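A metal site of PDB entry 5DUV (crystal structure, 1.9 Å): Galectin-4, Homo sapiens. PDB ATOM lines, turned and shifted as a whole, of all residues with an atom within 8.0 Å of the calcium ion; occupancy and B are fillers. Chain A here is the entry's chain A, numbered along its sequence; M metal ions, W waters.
The calcium ion is bound by water W2 (2.0 Å), O of Gly 70 (2.1 Å), OD1 of Asp 72 (2.2 Å), O of Phe 68 (2.3 Å), water W1 (2.3 Å) and water W3 (2.6 Å). The calcium ion has six donor atoms within binding distance.
Within 4 Å of the calcium ion: Phe 68, Gly 70 and Asp 72. The nearest printed residue that does not touch the calcium ion is Asp 69 (4.2 Å).
O of Lys 44 is in hydrogen-bond range of N of Phe 68 (2.8 Å).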
ATOM      1  N   MET A  43     -10.845  18.910  17.147  1.00  0.00           N
ATOM      2  CA  MET A  43     -11.361  17.838  17.992  1.00  0.00           C
ATOM      3  C   MET A  43     -10.676  17.746  19.351  1.00  0.00           C
ATOM      4  O   MET A  43      -9.451  17.625  19.436  1.00  0.00           O
ATOM      5  CB  MET A  43     -11.248  16.491  17.287  1.00  0.00           C
ATOM      6  CG  MET A  43     -11.708  15.333  18.163  1.00  0.00           C
ATOM      7  SD  MET A  43     -11.706  13.804  17.236  1.00  0.00           S
ATOM      8  CE  MET A  43     -11.475  12.596  18.542  1.00  0.00           C
ATOM      9  N   LYS A  44     -11.467  17.805  20.420  1.00  0.00           N
ATOM     10  CA  LYS A  44     -10.989  17.417  21.746  1.00  0.00           C
ATOM     11  C   LYS A  44     -11.443  15.986  22.041  1.00  0.00           C
ATOM     12  O   LYS A  44     -10.631  15.107  22.279  1.00  0.00           O
ATOM     13  CB  LYS A  44     -11.537  18.350  22.836  1.00  0.00           C
ATOM     14  CG  LYS A  44     -11.212  19.818  22.658  1.00  0.00           C
ATOM     15  CD  LYS A  44     -11.611  20.606  23.905  1.00  0.00           C
ATOM     16  CE  LYS A  44     -12.238  21.939  23.552  1.00  0.00           C
ATOM     17  NZ  LYS A  44     -11.261  22.906  22.996  1.00  0.00           N
ATOM     18  N   ARG A  67     -10.008  10.734  22.717  1.00  0.00           N
ATOM     19  CA  ARG A  67      -9.626  11.948  23.431  1.00  0.00           C
ATOM     20  C   ARG A  67      -8.262  12.427  22.981  1.00  0.00           C
ATOM     21  O   ARG A  67      -7.293  11.655  22.968  1.00  0.00           O
ATOM     22  CB  ARG A  67      -9.522  11.688  24.924  1.00  0.00           C
ATOM     23  CG  ARG A  67     -10.742  11.096  25.613  1.00  0.00           C
ATOM     24  CD  ARG A  67     -10.486  11.010  27.107  1.00  0.00           C
ATOM     25  NE  ARG A  67     -11.615  10.506  27.851  1.00  0.00           N
ATOM     26  CZ  ARG A  67     -11.595  10.265  29.155  1.00  0.00           C
ATOM     27  NH1 ARG A  67     -10.484  10.475  29.863  1.00  0.00           N
ATOM     28  NH2 ARG A  67     -12.685   9.813  29.750  1.00  0.00           N
ATOM     29  N   PHE A  68      -8.179  13.709  22.633  1.00  0.00           N
ATOM     30  CA  PHE A  68      -6.886  14.340  22.377  1.00  0.00           C
ATOM     31  C   PHE A  68      -6.302  15.025  23.608  1.00  0.00           C
ATOM     32  O   PHE A  68      -5.120  15.354  23.602  1.00  0.00           O
ATOM     33  CB  PHE A  68      -6.993  15.350  21.241  1.00  0.00           C
ATOM     34  CG  PHE A  68      -6.910  14.723  19.871  1.00  0.00           C
ATOM     35  CD1 PHE A  68      -5.678  14.354  19.341  1.00  0.00           C
ATOM     36  CD2 PHE A  68      -8.050  14.496  19.131  1.00  0.00           C
ATOM     37  CE1 PHE A  68      -5.604  13.780  18.086  1.00  0.00           C
ATOM     38  CE2 PHE A  68      -7.976  13.922  17.876  1.00  0.00           C
ATOM     39  CZ  PHE A  68      -6.750  13.558  17.358  1.00  0.00           C
ATOM     40  N   ASP A  69      -7.082  15.236  24.657  1.00  0.00           N
ATOM     41  CA  ASP A  69      -6.524  15.850  25.857  1.00  0.00           C
ATOM     42  C   ASP A  69      -5.516  14.890  26.488  1.00  0.00           C
ATOM     43  O   ASP A  69      -5.786  13.703  26.676  1.00  0.00           O
ATOM     44  CB  ASP A  69      -7.607  16.269  26.869  1.00  0.00           C
ATOM     45  CG  ASP A  69      -8.588  15.154  27.203  1.00  0.00           C
ATOM     46  OD1 ASP A  69      -9.429  14.831  26.340  1.00  0.00           O
ATOM     47  OD2 ASP A  69      -8.521  14.614  28.341  1.00  0.00           O
ATOM     48  N   GLY A  70      -4.342  15.413  26.803  1.00  0.00           N
ATOM     49  CA  GLY A  70      -3.255  14.596  27.332  1.00  0.00           C
ATOM     50  C   GLY A  70      -2.664  13.730  26.233  1.00  0.00           C
ATOM     51  O   GLY A  70      -2.674  14.120  25.061  1.00  0.00           O
ATOM     52  N   TRP A  71      -2.158  12.566  26.615  1.00  0.00           N
ATOM     53  CA  TRP A  71      -1.724  11.562  25.647  1.00  0.00           C
ATOM     54  C   TRP A  71      -2.934  11.189  24.789  1.00  0.00           C
ATOM     55  O   TRP A  71      -3.966  10.774  25.319  1.00  0.00           O
ATOM     56  CB  TRP A  71      -1.195  10.322  26.367  1.00  0.00           C
ATOM     57  CG  TRP A  71       0.298  10.184  26.364  1.00  0.00           C
ATOM     58  CD1 TRP A  71       1.189  10.945  27.074  1.00  0.00           C
ATOM     59  CD2 TRP A  71       1.083   9.222  25.639  1.00  0.00           C
ATOM     60  NE1 TRP A  71       2.465  10.523  26.830  1.00  0.00           N
ATOM     61  CE2 TRP A  71       2.436   9.468  25.957  1.00  0.00           C
ATOM     62  CE3 TRP A  71       0.767   8.178  24.772  1.00  0.00           C
ATOM     63  CZ2 TRP A  71       3.476   8.699  25.422  1.00  0.00           C
ATOM     64  CZ3 TRP A  71       1.794   7.426  24.241  1.00  0.00           C
ATOM     65  CH2 TRP A  71       3.130   7.686  24.570  1.00  0.00           C
ATOM     66  N   ASP A  72      -2.806  11.322  23.483  1.00  0.00           N
ATOM     67  CA  ASP A  72      -3.902  10.967  22.585  1.00  0.00           C
ATOM     68  C   ASP A  72      -4.270   9.494  22.812  1.00  0.00           C
ATOM     69  O   ASP A  72      -3.410   8.616  22.812  1.00  0.00           O
ATOM     70  CB  ASP A  72      -3.529  11.234  21.123  1.00  0.00           C
ATOM     71  CG  ASP A  72      -3.113  12.677  20.889  1.00  0.00           C
ATOM     72  OD1 ASP A  72      -3.184  13.478  21.828  1.00  0.00           O
ATOM     73  OD2 ASP A  72      -2.710  13.015  19.753  1.00  0.00           O
ATOM     74  N   LYS A  73      -5.550   9.237  23.035  1.00  0.00           N
ATOM     75  CA  LYS A  73      -5.972   7.927  23.492  1.00  0.00           C
ATOM     76  C   LYS A  73      -7.442   7.696  23.240  1.00  0.00           C
ATOM     77  O   LYS A  73      -8.164   8.599  22.815  1.00  0.00           O
ATOM     78  CB  LYS A  73      -5.669   7.776  24.987  1.00  0.00           C
ATOM     79  CG  LYS A  73      -6.487   8.684  25.897  1.00  0.00           C
ATOM     80  CD  LYS A  73      -6.023   8.529  27.349  1.00  0.00           C
ATOM     81  CE  LYS A  73      -6.136   9.811  28.141  1.00  0.00           C
ATOM     82  NZ  LYS A  73      -5.205  10.890  27.699  1.00  0.00           N
ATOM     83  N   MET A  93      -4.272   6.753  19.050  1.00  0.00           N
ATOM     84  CA  MET A  93      -5.346   7.549  18.469  1.00  0.00           C
ATOM     85  C   MET A  93      -5.472   7.248  16.979  1.00  0.00           C
ATOM     86  O   MET A  93      -4.566   7.564  16.199  1.00  0.00           O
ATOM     87  CB  MET A  93      -5.084   9.040  18.688  1.00  0.00           C
ATOM     88  CG  MET A  93      -5.980   9.973  17.902  1.00  0.00           C
ATOM     89  SD  MET A  93      -7.712   9.851  18.345  1.00  0.00           S
ATOM     90  CE  MET A  93      -7.644  10.461  20.025  1.00  0.00           C
ATOM     91  N   LYS A  97      -7.541  14.912  13.279  1.00  0.00           N
ATOM     92  CA  LYS A  97      -8.242  16.174  13.134  1.00  0.00           C
ATOM     93  C   LYS A  97      -8.452  16.541  11.671  1.00  0.00           C
ATOM     94  O   LYS A  97      -7.498  16.607  10.889  1.00  0.00           O
ATOM     95  CB  LYS A  97      -7.460  17.269  13.848  1.00  0.00           C
ATOM     96  CG  LYS A  97      -7.392  17.043  15.342  1.00  0.00           C
ATOM     97  CD  LYS A  97      -6.625  18.141  16.040  1.00  0.00           C
ATOM     98  CE  LYS A  97      -6.457  17.799  17.497  1.00  0.00           C
ATOM     99  NZ  LYS A  97      -5.875  18.928  18.264  1.00  0.00           N
HETATM  100 CA    CA M   1      -2.873  15.164  23.223  1.00  0.00          CA
HETATM  101  O   HOH W   1      -0.800  14.504  22.451  1.00  0.00           O
HETATM  102  O   HOH W   2      -3.149  16.550  21.793  1.00  0.00           O
HETATM  103  O   HOH W   3      -2.590  17.167  24.917  1.00  0.00           O
